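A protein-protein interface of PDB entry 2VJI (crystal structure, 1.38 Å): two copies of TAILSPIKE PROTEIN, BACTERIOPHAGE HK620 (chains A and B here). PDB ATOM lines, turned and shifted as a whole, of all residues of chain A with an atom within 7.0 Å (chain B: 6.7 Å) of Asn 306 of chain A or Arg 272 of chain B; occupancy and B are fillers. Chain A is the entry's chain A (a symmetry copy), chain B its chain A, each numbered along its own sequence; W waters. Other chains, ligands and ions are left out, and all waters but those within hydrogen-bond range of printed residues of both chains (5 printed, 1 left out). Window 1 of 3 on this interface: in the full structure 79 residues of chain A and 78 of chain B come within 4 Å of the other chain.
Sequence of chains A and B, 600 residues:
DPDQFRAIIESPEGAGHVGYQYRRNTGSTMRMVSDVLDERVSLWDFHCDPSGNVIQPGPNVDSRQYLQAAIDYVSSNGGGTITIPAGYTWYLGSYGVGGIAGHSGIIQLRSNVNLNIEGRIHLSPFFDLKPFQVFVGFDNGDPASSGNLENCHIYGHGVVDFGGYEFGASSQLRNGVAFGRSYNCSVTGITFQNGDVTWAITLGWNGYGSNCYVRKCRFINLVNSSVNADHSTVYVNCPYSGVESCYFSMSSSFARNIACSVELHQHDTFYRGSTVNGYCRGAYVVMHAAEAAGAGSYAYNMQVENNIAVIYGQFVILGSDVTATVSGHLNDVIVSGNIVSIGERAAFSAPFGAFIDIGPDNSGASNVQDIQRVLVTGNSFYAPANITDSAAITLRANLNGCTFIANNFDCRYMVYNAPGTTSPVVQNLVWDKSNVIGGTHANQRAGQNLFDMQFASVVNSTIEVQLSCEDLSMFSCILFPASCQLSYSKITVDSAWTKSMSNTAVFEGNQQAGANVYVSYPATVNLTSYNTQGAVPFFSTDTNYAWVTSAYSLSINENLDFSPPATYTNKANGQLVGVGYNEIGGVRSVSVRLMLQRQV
The side-chain hydroxyl (OG) of Ser 245 of chain A lies within hydrogen-bond range of the side-chain carboxylate (OE1) of Glu 244 of chain B (3.2 Å). The side-chain amide oxygen (OE1) of Gln 303 of chain B lies close to the backbone carbonyl oxygen (O) of Asn 307 of chain A. The side-chain amide oxygen (OE1) of Gln 303 of chain B sits close to the backbone carbonyl oxygen (O) of Gly 337 of chain A. The side-chain carboxylate of Glu 305 of chain B sits close to the side-chain amide oxygen of Asn 306 of chain A (3.1 Å). The side-chain amide nitrogen of Asn 306 of chain A sits close to the side-chain amide nitrogen of Asn 306 of chain B, at 3.0 Å. The side-chain carboxylate of Glu 305 of chain B lies close to the backbone carbonyl oxygen of Gly 337 of chain A. The side-chain amide oxygen (OE1) of Gln 303 of chain B sits close to the backbone carbonyl oxygen (O) of Asn 306 of chain A (3.4 Å). The backbone carbonyl oxygen of Gly 273 of chain A sits at hydrogen-bond distance from the guanidinium group of Arg 272 of chain B.
N of Gly 273 of chain A sits at hydrogen-bond distance from O of Glu 305 of chain A, 3.0 Å away. The backbone NH of Val 304 of chain B is in hydrogen-bond range of the backbone carbonyl oxygen of Ile 334 of chain B, 2.9 Å away.
Arg 272 of chain B touches Asn 306 of chain A (NH1 to O, 3.8 Å). Ile 308 of chain A touches Gln 303 of chain B. Ile 334 of chain B touches Gly 337 of chain A. Ile 339 of chain A touches Ile 334 of chain B (CD1 to N, 3.9 Å). Ile 334 of chain B touches Gly 378 of chain A.
Of the printed residues of chain B, Ser 245 of chain A touches Glu 244 (3.2 Å). Of the printed residues of chain B, Asn 306 of chain A touches Arg 272 (3.8 Å), Gln 303 (3.4 Å), Glu 305 (3.1 Å) and Asn 306 (3.0 Å). Printed residues of chain A within 4 Å of Glu 244 of chain B: Ser 245 (3.2 Å). Arg 272 of chain B touches two residues of chain A.
Of the 19 printed residues of chain B, 6 touch a printed residue of chain A. Hydrophobic or aromatic side chains of chain B within 4 Å of the printed part of chain A: Ile 334. Along chain B the printed residues that touch a printed residue of chain A span positions 244 to 334. Of the 20 printed residues of chain A, 8 touch a printed residue of chain B.
Ser 245 of chain A touches Glu 244 of chain B, but with the chains exchanged Glu 244 of chain A does not touch Ser 245 of chain B (7.0 Å). Asn 306 of chain A touches Arg 272 of chain B, but with the chains exchanged Arg 272 of chain A does not touch Asn 306 of chain B (7.5 Å). Asn 306 of chain B touches its own counterpart, Asn 306 of chain A.
Water W5 bridges the backbone carbonyl oxygen (O) of Gly 378 of chain A (2.7 Å) and the side-chain hydroxyl (OG) of Ser 336 of chain B (3.2 Å).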
ATOM      1  N   GLU A 244      29.996  12.934  19.879  1.00  0.00           N
ATOM      2  CA  GLU A 244      29.085  12.437  18.870  1.00  0.00           C
ATOM      3  C   GLU A 244      28.299  13.559  18.226  1.00  0.00           C
ATOM      4  O   GLU A 244      27.818  14.467  18.896  1.00  0.00           O
ATOM      5  CB  GLU A 244      28.119  11.415  19.507  1.00  0.00           C
ATOM      6  CG  GLU A 244      27.202  10.684  18.539  1.00  0.00           C
ATOM      7  CD  GLU A 244      26.563   9.436  19.155  1.00  0.00           C
ATOM      8  OE1 GLU A 244      26.676   9.249  20.388  1.00  0.00           O
ATOM      9  OE2 GLU A 244      25.950   8.646  18.400  1.00  0.00           O
ATOM     10  N   SER A 245      28.145  13.486  16.911  1.00  0.00           N
ATOM     11  CA  SER A 245      27.280  14.388  16.142  1.00  0.00           C
ATOM     12  C   SER A 245      27.545  15.867  16.349  1.00  0.00           C
ATOM     13  O   SER A 245      26.622  16.661  16.526  1.00  0.00           O
ATOM     14  CB  SER A 245      25.814  14.068  16.459  1.00  0.00           C
ATOM     15  OG  SER A 245      25.506  12.701  16.198  1.00  0.00           O
ATOM     16  N   CYS A 246      28.816  16.217  16.344  1.00  0.00           N
ATOM     17  CA  CYS A 246      29.229  17.609  16.473  1.00  0.00           C
ATOM     18  C   CYS A 246      29.702  18.172  15.137  1.00  0.00           C
ATOM     19  O   CYS A 246      29.895  17.438  14.155  1.00  0.00           O
ATOM     20  CB  CYS A 246      30.327  17.782  17.537  1.00  0.00           C
ATOM     21  SG  CYS A 246      29.764  17.406  19.232  1.00  0.00           S
ATOM     22  N   TYR A 271      34.675   8.912  18.983  1.00  0.00           N
ATOM     23  CA  TYR A 271      34.485  10.130  18.207  1.00  0.00           C
ATOM     24  C   TYR A 271      33.705   9.703  16.988  1.00  0.00           C
ATOM     25  O   TYR A 271      34.255   9.058  16.107  1.00  0.00           O
ATOM     26  CB  TYR A 271      35.814  10.747  17.829  1.00  0.00           C
ATOM     27  CG  TYR A 271      35.724  11.992  16.985  1.00  0.00           C
ATOM     28  CD1 TYR A 271      34.637  12.846  17.066  1.00  0.00           C
ATOM     29  CD2 TYR A 271      36.803  12.379  16.230  1.00  0.00           C
ATOM     30  CE1 TYR A 271      34.593  14.026  16.325  1.00  0.00           C
ATOM     31  CE2 TYR A 271      36.765  13.549  15.489  1.00  0.00           C
ATOM     32  CZ  TYR A 271      35.659  14.367  15.556  1.00  0.00           C
ATOM     33  OH  TYR A 271      35.630  15.544  14.822  1.00  0.00           O
ATOM     34  N   ARG A 272      32.417  10.027  16.947  1.00  0.00           N
ATOM     35  CA  ARG A 272      31.569   9.549  15.872  1.00  0.00           C
ATOM     36  C   ARG A 272      30.666  10.599  15.281  1.00  0.00           C
ATOM     37  O   ARG A 272      30.270  11.546  15.952  1.00  0.00           O
ATOM     38  CB  ARG A 272      30.642   8.429  16.368  1.00  0.00           C
ATOM     39  CG  ARG A 272      31.291   7.215  17.012  1.00  0.00           C
ATOM     40  CD  ARG A 272      30.224   6.136  17.252  1.00  0.00           C
ATOM     41  NE  ARG A 272      29.251   6.526  18.274  1.00  0.00           N
ATOM     42  CZ  ARG A 272      29.151   6.036  19.517  1.00  0.00           C
ATOM     43  NH1 ARG A 272      29.954   5.081  19.987  1.00  0.00           N
ATOM     44  NH2 ARG A 272      28.197   6.509  20.303  1.00  0.00           N
ATOM     45  N   GLY A 273      30.291  10.361  14.028  1.00  0.00           N
ATOM     46  CA  GLY A 273      29.226  11.095  13.361  1.00  0.00           C
ATOM     47  C   GLY A 273      29.348  12.594  13.293  1.00  0.00           C
ATOM     48  O   GLY A 273      28.343  13.301  13.238  1.00  0.00           O
ATOM     49  N   SER A 274      30.575  13.089  13.279  1.00  0.00           N
ATOM     50  CA  SER A 274      30.823  14.508  13.303  1.00  0.00           C
ATOM     51  C   SER A 274      31.374  15.003  11.993  1.00  0.00           C
ATOM     52  O   SER A 274      31.830  14.213  11.174  1.00  0.00           O
ATOM     53  CB  SER A 274      31.786  14.802  14.436  1.00  0.00           C
ATOM     54  OG  SER A 274      31.204  14.428  15.700  1.00  0.00           O
ATOM     55  N   THR A 275      31.303  16.314  11.808  1.00  0.00           N
ATOM     56  CA  THR A 275      31.777  16.967  10.604  1.00  0.00           C
ATOM     57  C   THR A 275      32.833  18.002  10.991  1.00  0.00           C
ATOM     58  O   THR A 275      32.647  18.777  11.946  1.00  0.00           O
ATOM     59  CB  THR A 275      30.622  17.607   9.812  1.00  0.00           C
ATOM     60  OG1 THR A 275      29.712  16.588   9.373  1.00  0.00           O
ATOM     61  CG2 THR A 275      31.140  18.368   8.599  1.00  0.00           C
ATOM     62  N   VAL A 304      36.847   5.751  16.110  1.00  0.00           N
ATOM     63  CA  VAL A 304      36.720   6.957  15.286  1.00  0.00           C
ATOM     64  C   VAL A 304      35.890   6.482  14.099  1.00  0.00           C
ATOM     65  O   VAL A 304      36.410   5.835  13.195  1.00  0.00           O
ATOM     66  CB  VAL A 304      38.090   7.544  14.857  1.00  0.00           C
ATOM     67  CG1 VAL A 304      37.918   8.770  13.969  1.00  0.00           C
ATOM     68  CG2 VAL A 304      38.941   7.887  16.067  1.00  0.00           C
ATOM     69  N   GLU A 305      34.600   6.815  14.096  1.00  0.00           N
ATOM     70  CA  GLU A 305      33.711   6.297  13.092  1.00  0.00           C
ATOM     71  C   GLU A 305      32.723   7.281  12.508  1.00  0.00           C
ATOM     72  O   GLU A 305      32.196   8.141  13.199  1.00  0.00           O
ATOM     73  CB  GLU A 305      32.915   5.099  13.647  1.00  0.00           C
ATOM     74  CG  GLU A 305      33.740   3.846  13.908  1.00  0.00           C
ATOM     75  CD  GLU A 305      32.962   2.692  14.516  1.00  0.00           C
ATOM     76  OE1 GLU A 305      31.953   2.935  15.187  1.00  0.00           O
ATOM     77  OE2 GLU A 305      33.399   1.546  14.356  1.00  0.00           O
ATOM     78  N   ASN A 306      32.468   7.118  11.214  1.00  0.00           N
ATOM     79  CA  ASN A 306      31.388   7.803  10.523  1.00  0.00           C
ATOM     80  C   ASN A 306      31.485   9.313  10.565  1.00  0.00           C
ATOM     81  O   ASN A 306      30.473  10.007  10.644  1.00  0.00           O
ATOM     82  CB  ASN A 306      30.029   7.331  11.060  1.00  0.00           C
ATOM     83  CG  ASN A 306      29.807   5.847  10.851  1.00  0.00           C
ATOM     84  OD1 ASN A 306      30.496   5.207  10.070  1.00  0.00           O
ATOM     85  ND2 ASN A 306      28.823   5.301  11.544  1.00  0.00           N
ATOM     86  N   ASN A 307      32.713   9.821  10.558  1.00  0.00           N
ATOM     87  CA  ASN A 307      32.939  11.250  10.512  1.00  0.00           C
ATOM     88  C   ASN A 307      33.178  11.710   9.073  1.00  0.00           C
ATOM     89  O   ASN A 307      33.536  10.927   8.193  1.00  0.00           O
ATOM     90  CB  ASN A 307      34.119  11.629  11.388  1.00  0.00           C
ATOM     91  CG  ASN A 307      33.931  11.176  12.813  1.00  0.00           C
ATOM     92  OD1 ASN A 307      33.073  11.706  13.529  1.00  0.00           O
ATOM     93  ND2 ASN A 307      34.728  10.217  13.241  1.00  0.00           N
ATOM     94  N   ILE A 308      32.977  13.001   8.855  1.00  0.00           N
ATOM     95  CA  ILE A 308      33.177  13.660   7.577  1.00  0.00           C
ATOM     96  C   ILE A 308      34.192  14.775   7.832  1.00  0.00           C
ATOM     97  O   ILE A 308      34.003  15.562   8.752  1.00  0.00           O
ATOM     98  CB  ILE A 308      31.864  14.271   7.083  1.00  0.00           C
ATOM     99  CG1 ILE A 308      30.788  13.210   6.884  1.00  0.00           C
ATOM    100  CG2 ILE A 308      32.080  15.025   5.790  1.00  0.00           C
ATOM    101  CD1 ILE A 308      29.408  13.829   6.547  1.00  0.00           C
ATOM    102  N   VAL A 335      38.967   2.542  13.182  1.00  0.00           N
ATOM    103  CA  VAL A 335      38.756   3.738  12.379  1.00  0.00           C
ATOM    104  C   VAL A 335      37.977   3.292  11.152  1.00  0.00           C
ATOM    105  O   VAL A 335      38.512   2.603  10.288  1.00  0.00           O
ATOM    106  CB  VAL A 335      40.085   4.384  11.987  1.00  0.00           C
ATOM    107  CG1 VAL A 335      39.851   5.638  11.191  1.00  0.00           C
ATOM    108  CG2 VAL A 335      40.916   4.691  13.224  1.00  0.00           C
ATOM    109  N   SER A 336      36.699   3.655  11.085  1.00  0.00           N
ATOM    110  CA  SER A 336      35.874   3.147  10.006  1.00  0.00           C
ATOM    111  C   SER A 336      34.731   4.057   9.619  1.00  0.00           C
ATOM    112  O   SER A 336      34.217   4.832  10.419  1.00  0.00           O
ATOM    113  CB  SER A 336      35.335   1.763  10.372  1.00  0.00           C
ATOM    114  OG  SER A 336      34.428   1.857  11.434  1.00  0.00           O
ATOM    115  N   GLY A 337      34.363   3.963   8.348  1.00  0.00           N
ATOM    116  CA  GLY A 337      33.256   4.731   7.815  1.00  0.00           C
ATOM    117  C   GLY A 337      33.441   6.217   7.679  1.00  0.00           C
ATOM    118  O   GLY A 337      32.468   6.957   7.495  1.00  0.00           O
ATOM    119  N   ASN A 338      34.683   6.684   7.754  1.00  0.00           N
ATOM    120  CA  ASN A 338      34.973   8.095   7.646  1.00  0.00           C
ATOM    121  C   ASN A 338      35.228   8.496   6.193  1.00  0.00           C
ATOM    122  O   ASN A 338      35.809   7.732   5.421  1.00  0.00           O
ATOM    123  CB  ASN A 338      36.230   8.409   8.451  1.00  0.00           C
ATOM    124  CG  ASN A 338      36.092   8.029   9.922  1.00  0.00           C
ATOM    125  OD1 ASN A 338      35.442   8.727  10.693  1.00  0.00           O
ATOM    126  ND2 ASN A 338      36.734   6.942  10.319  1.00  0.00           N
ATOM    127  N   ILE A 339      34.795   9.691   5.835  1.00  0.00           N
ATOM    128  CA  ILE A 339      35.061  10.258   4.521  1.00  0.00           C
ATOM    129  C   ILE A 339      35.880  11.512   4.753  1.00  0.00           C
ATOM    130  O   ILE A 339      35.435  12.446   5.421  1.00  0.00           O
ATOM    131  CB  ILE A 339      33.792  10.393   3.646  1.00  0.00           C
ATOM    132  CG1 ILE A 339      34.187  10.848   2.241  1.00  0.00           C
ATOM    133  CG2 ILE A 339      32.755  11.276   4.272  1.00  0.00           C
ATOM    134  CD1 ILE A 339      33.335  10.227   1.173  1.00  0.00           C
ATOM    135  N   GLY A 378      36.883   0.475   5.595  1.00  0.00           N
ATOM    136  CA  GLY A 378      35.717   1.144   5.068  1.00  0.00           C
ATOM    137  C   GLY A 378      35.751   2.666   5.113  1.00  0.00           C
ATOM    138  O   GLY A 378      34.721   3.297   5.338  1.00  0.00           O
ATOM    139  N   ASN A 379      36.925   3.247   4.915  1.00  0.00           N
ATOM    140  CA  ASN A 379      37.074   4.696   4.865  1.00  0.00           C
ATOM    141  C   ASN A 379      37.403   5.137   3.443  1.00  0.00           C
ATOM    142  O   ASN A 379      37.911   4.352   2.648  1.00  0.00           O
ATOM    143  CB  ASN A 379      38.245   5.120   5.749  1.00  0.00           C
ATOM    144  CG  ASN A 379      38.092   4.687   7.190  1.00  0.00           C
ATOM    145  OD1 ASN A 379      37.336   5.305   7.946  1.00  0.00           O
ATOM    146  ND2 ASN A 379      38.837   3.654   7.606  1.00  0.00           N
ATOM    147  N   GLY B 242      22.023  17.463   7.763  1.00  0.00           N
ATOM    148  CA  GLY B 242      21.697  16.065   7.612  1.00  0.00           C
ATOM    149  C   GLY B 242      20.521  15.570   8.411  1.00  0.00           C
ATOM    150  O   GLY B 242      19.881  16.310   9.151  1.00  0.00           O
ATOM    151  N   VAL B 243      20.265  14.282   8.223  1.00  0.00           N
ATOM    152  CA  VAL B 243      19.173  13.540   8.819  1.00  0.00           C
ATOM    153  C   VAL B 243      19.763  12.387   9.586  1.00  0.00           C
ATOM    154  O   VAL B 243      20.571  11.637   9.036  1.00  0.00           O
ATOM    155  CB  VAL B 243      18.253  12.978   7.717  1.00  0.00           C
ATOM    156  CG1 VAL B 243      17.114  12.136   8.310  1.00  0.00           C
ATOM    157  CG2 VAL B 243      17.724  14.114   6.872  1.00  0.00           C
ATOM    158  N   GLU B 244      19.342  12.236  10.841  1.00  0.00           N
ATOM    159  CA  GLU B 244      19.841  11.186  11.704  1.00  0.00           C
ATOM    160  C   GLU B 244      18.739  10.600  12.562  1.00  0.00           C
ATOM    161  O   GLU B 244      17.911  11.317  13.114  1.00  0.00           O
ATOM    162  CB  GLU B 244      20.965  11.745  12.601  1.00  0.00           C
ATOM    163  CG  GLU B 244      21.698  10.721  13.453  1.00  0.00           C
ATOM    164  CD  GLU B 244      23.024  11.250  14.006  1.00  0.00           C
ATOM    165  OE1 GLU B 244      23.279  12.471  13.893  1.00  0.00           O
ATOM    166  OE2 GLU B 244      23.808  10.441  14.553  1.00  0.00           O
ATOM    167  N   SER B 245      18.741   9.281  12.697  1.00  0.00           N
ATOM    168  CA  SER B 245      17.857   8.557  13.617  1.00  0.00           C
ATOM    169  C   SER B 245      16.379   8.857  13.461  1.00  0.00           C
ATOM    170  O   SER B 245      15.664   9.070  14.440  1.00  0.00           O
ATOM    171  CB  SER B 245      18.299   8.832  15.059  1.00  0.00           C
ATOM    172  OG  SER B 245      19.666   8.483  15.265  1.00  0.00           O
ATOM    173  N   CYS B 246      15.940   8.892  12.219  1.00  0.00           N
ATOM    174  CA  CYS B 246      14.532   9.111  11.907  1.00  0.00           C
ATOM    175  C   CYS B 246      13.855   7.819  11.463  1.00  0.00           C
ATOM    176  O   CYS B 246      14.512   6.797  11.209  1.00  0.00           O
ATOM    177  CB  CYS B 246      14.348  10.200  10.836  1.00  0.00           C
ATOM    178  SG  CYS B 246      14.867  11.860  11.387  1.00  0.00           S
ATOM    179  N   PHE B 270      24.579  14.342   5.248  1.00  0.00           N
ATOM    180  CA  PHE B 270      24.494  12.959   5.669  1.00  0.00           C
ATOM    181  C   PHE B 270      23.086  12.486   5.919  1.00  0.00           C
ATOM    182  O   PHE B 270      22.168  13.276   6.192  1.00  0.00           O
ATOM    183  CB  PHE B 270      25.326  12.747   6.941  1.00  0.00           C
ATOM    184  CG  PHE B 270      24.887  13.583   8.102  1.00  0.00           C
ATOM    185  CD1 PHE B 270      23.854  13.171   8.936  1.00  0.00           C
ATOM    186  CD2 PHE B 270      25.502  14.801   8.352  1.00  0.00           C
ATOM    187  CE1 PHE B 270      23.462  13.959  10.024  1.00  0.00           C
ATOM    188  CE2 PHE B 270      25.105  15.598   9.420  1.00  0.00           C
ATOM    189  CZ  PHE B 270      24.086  15.169  10.250  1.00  0.00           C
ATOM    190  N   TYR B 271      22.958  11.164   5.876  1.00  0.00           N
ATOM    191  CA  TYR B 271      21.713  10.461   6.145  1.00  0.00           C
ATOM    192  C   TYR B 271      22.117   9.207   6.880  1.00  0.00           C
ATOM    193  O   TYR B 271      22.665   8.296   6.277  1.00  0.00           O
ATOM    194  CB  TYR B 271      20.980  10.140   4.861  1.00  0.00           C
ATOM    195  CG  TYR B 271      19.695   9.373   5.031  1.00  0.00           C
ATOM    196  CD1 TYR B 271      18.927   9.490   6.178  1.00  0.00           C
ATOM    197  CD2 TYR B 271      19.186   8.659   3.975  1.00  0.00           C
ATOM    198  CE1 TYR B 271      17.710   8.822   6.299  1.00  0.00           C
ATOM    199  CE2 TYR B 271      17.978   7.990   4.090  1.00  0.00           C
ATOM    200  CZ  TYR B 271      17.246   8.091   5.253  1.00  0.00           C
ATOM    201  OH  TYR B 271      16.031   7.430   5.358  1.00  0.00           O
ATOM    202  N   ARG B 272      21.884   9.167   8.188  1.00  0.00           N
ATOM    203  CA  ARG B 272      22.353   8.053   8.989  1.00  0.00           C
ATOM    204  C   ARG B 272      21.335   7.514   9.959  1.00  0.00           C
ATOM    205  O   ARG B 272      20.461   8.236  10.428  1.00  0.00           O
ATOM    206  CB  ARG B 272      23.565   8.467   9.838  1.00  0.00           C
ATOM    207  CG  ARG B 272      24.768   9.045   9.109  1.00  0.00           C
ATOM    208  CD  ARG B 272      25.932   9.203  10.100  1.00  0.00           C
ATOM    209  NE  ARG B 272      25.676  10.233  11.108  1.00  0.00           N
ATOM    210  CZ  ARG B 272      26.248  11.441  11.185  1.00  0.00           C
ATOM    211  NH1 ARG B 272      27.170  11.864  10.320  1.00  0.00           N
ATOM    212  NH2 ARG B 272      25.893  12.242  12.178  1.00  0.00           N
ATOM    213  N   GLY B 273      21.521   6.244  10.303  1.00  0.00           N
ATOM    214  CA  GLY B 273      20.825   5.608  11.412  1.00  0.00           C
ATOM    215  C   GLY B 273      19.320   5.633  11.397  1.00  0.00           C
ATOM    216  O   GLY B 273      18.684   5.608  12.449  1.00  0.00           O
ATOM    217  N   SER B 274      18.739   5.668  10.208  1.00  0.00           N
ATOM    218  CA  SER B 274      17.310   5.781  10.063  1.00  0.00           C
ATOM    219  C   SER B 274      16.697   4.512   9.537  1.00  0.00           C
ATOM    220  O   SER B 274      17.400   3.653   9.017  1.00  0.00           O
ATOM    221  CB  SER B 274      17.019   6.944   9.136  1.00  0.00           C
ATOM    222  OG  SER B 274      17.510   8.173   9.702  1.00  0.00           O
ATOM    223  N   THR B 275      15.385   4.407   9.699  1.00  0.00           N
ATOM    224  CA  THR B 275      14.626   3.251   9.261  1.00  0.00           C
ATOM    225  C   THR B 275      13.545   3.716   8.286  1.00  0.00           C
ATOM    226  O   THR B 275      12.846   4.714   8.536  1.00  0.00           O
ATOM    227  CB  THR B 275      14.023   2.483  10.451  1.00  0.00           C
ATOM    228  OG1 THR B 275      15.075   1.970  11.282  1.00  0.00           O
ATOM    229  CG2 THR B 275      13.153   1.327   9.977  1.00  0.00           C
ATOM    230  N   GLN B 303      27.294  11.257   2.938  1.00  0.00           N
ATOM    231  CA  GLN B 303      27.312  10.020   3.693  1.00  0.00           C
ATOM    232  C   GLN B 303      25.913   9.407   3.801  1.00  0.00           C
ATOM    233  O   GLN B 303      24.975  10.087   4.206  1.00  0.00           O
ATOM    234  CB  GLN B 303      27.837  10.376   5.091  1.00  0.00           C
ATOM    235  CG  GLN B 303      28.780   9.404   5.752  1.00  0.00           C
ATOM    236  CD  GLN B 303      29.413   9.986   7.017  1.00  0.00           C
ATOM    237  OE1 GLN B 303      30.597   9.762   7.300  1.00  0.00           O
ATOM    238  NE2 GLN B 303      28.636  10.761   7.758  1.00  0.00           N
ATOM    239  N   VAL B 304      25.774   8.135   3.455  1.00  0.00           N
ATOM    240  CA  VAL B 304      24.531   7.384   3.660  1.00  0.00           C
ATOM    241  C   VAL B 304      24.990   6.158   4.442  1.00  0.00           C
ATOM    242  O   VAL B 304      25.540   5.224   3.867  1.00  0.00           O
ATOM    243  CB  VAL B 304      23.823   7.012   2.331  1.00  0.00           C
ATOM    244  CG1 VAL B 304      22.560   6.198   2.582  1.00  0.00           C
ATOM    245  CG2 VAL B 304      23.496   8.252   1.518  1.00  0.00           C
ATOM    246  N   GLU B 305      24.749   6.157   5.752  1.00  0.00           N
ATOM    247  CA  GLU B 305      25.266   5.111   6.591  1.00  0.00           C
ATOM    248  C   GLU B 305      24.320   4.575   7.641  1.00  0.00           C
ATOM    249  O   GLU B 305      23.544   5.308   8.235  1.00  0.00           O
ATOM    250  CB  GLU B 305      26.550   5.580   7.304  1.00  0.00           C
ATOM    251  CG  GLU B 305      27.755   5.776   6.394  1.00  0.00           C
ATOM    252  CD  GLU B 305      28.996   6.302   7.093  1.00  0.00           C
ATOM    253  OE1 GLU B 305      28.869   6.971   8.125  1.00  0.00           O
ATOM    254  OE2 GLU B 305      30.097   6.078   6.574  1.00  0.00           O
ATOM    255  N   ASN B 306      24.421   3.269   7.871  1.00  0.00           N
ATOM    256  CA  ASN B 306      23.773   2.605   8.990  1.00  0.00           C
ATOM    257  C   ASN B 306      22.266   2.741   9.003  1.00  0.00           C
ATOM    258  O   ASN B 306      21.651   2.848  10.063  1.00  0.00           O
ATOM    259  CB  ASN B 306      24.373   3.093  10.317  1.00  0.00           C
ATOM    260  CG  ASN B 306      25.853   2.790  10.431  1.00  0.00           C
ATOM    261  OD1 ASN B 306      26.393   1.982   9.689  1.00  0.00           O
ATOM    262  ND2 ASN B 306      26.509   3.435  11.379  1.00  0.00           N
ATOM    263  N   ASN B 307      21.672   2.782   7.814  1.00  0.00           N
ATOM    264  CA  ASN B 307      20.230   2.828   7.692  1.00  0.00           C
ATOM    265  C   ASN B 307      19.666   1.423   7.471  1.00  0.00           C
ATOM    266  O   ASN B 307      20.365   0.502   7.050  1.00  0.00           O
ATOM    267  CB  ASN B 307      19.823   3.742   6.550  1.00  0.00           C
ATOM    268  CG  ASN B 307      20.375   5.133   6.720  1.00  0.00           C
ATOM    269  OD1 ASN B 307      19.954   5.868   7.620  1.00  0.00           O
ATOM    270  ND2 ASN B 307      21.301   5.514   5.860  1.00  0.00           N
ATOM    271  N   ILE B 334      30.121   8.122   0.542  1.00  0.00           N
ATOM    272  CA  ILE B 334      30.261   6.826   1.185  1.00  0.00           C
ATOM    273  C   ILE B 334      28.879   6.284   1.494  1.00  0.00           C
ATOM    274  O   ILE B 334      28.062   6.970   2.098  1.00  0.00           O
ATOM    275  CB  ILE B 334      31.178   6.896   2.426  1.00  0.00           C
ATOM    276  CG1 ILE B 334      31.452   5.509   2.978  1.00  0.00           C
ATOM    277  CG2 ILE B 334      30.626   7.835   3.480  1.00  0.00           C
ATOM    278  CD1 ILE B 334      32.650   5.491   3.894  1.00  0.00           C
ATOM    279  N   SER B 336      27.559   2.989   3.401  1.00  0.00           N
ATOM    280  CA  SER B 336      28.058   1.870   4.177  1.00  0.00           C
ATOM    281  C   SER B 336      27.208   1.522   5.378  1.00  0.00           C
ATOM    282  O   SER B 336      26.522   2.361   5.955  1.00  0.00           O
ATOM    283  CB  SER B 336      29.495   2.143   4.619  1.00  0.00           C
ATOM    284  OG  SER B 336      29.532   3.195   5.540  1.00  0.00           O
ATOM    285  N   ASN B 338      24.480  -0.179   5.596  1.00  0.00           N
ATOM    286  CA  ASN B 338      23.049  -0.197   5.407  1.00  0.00           C
ATOM    287  C   ASN B 338      22.541  -1.619   5.168  1.00  0.00           C
ATOM    288  O   ASN B 338      23.213  -2.427   4.525  1.00  0.00           O
ATOM    289  CB  ASN B 338      22.698   0.644   4.184  1.00  0.00           C
ATOM    290  CG  ASN B 338      23.177   2.087   4.309  1.00  0.00           C
ATOM    291  OD1 ASN B 338      22.575   2.890   5.016  1.00  0.00           O
ATOM    292  ND2 ASN B 338      24.238   2.427   3.595  1.00  0.00           N
HETATM  293  O   HOH W   1      29.068   2.940   8.215  1.00  0.00           O
HETATM  294  O   HOH W   2      23.242   9.337  17.286  1.00  0.00           O
HETATM  295  O   HOH W   3      28.201  15.012  11.052  1.00  0.00           O
HETATM  296  O   HOH W   4      26.798   9.626  15.480  1.00  0.00           O
HETATM  297  O   HOH W   5      32.436   2.050   6.071  1.00  0.00           O
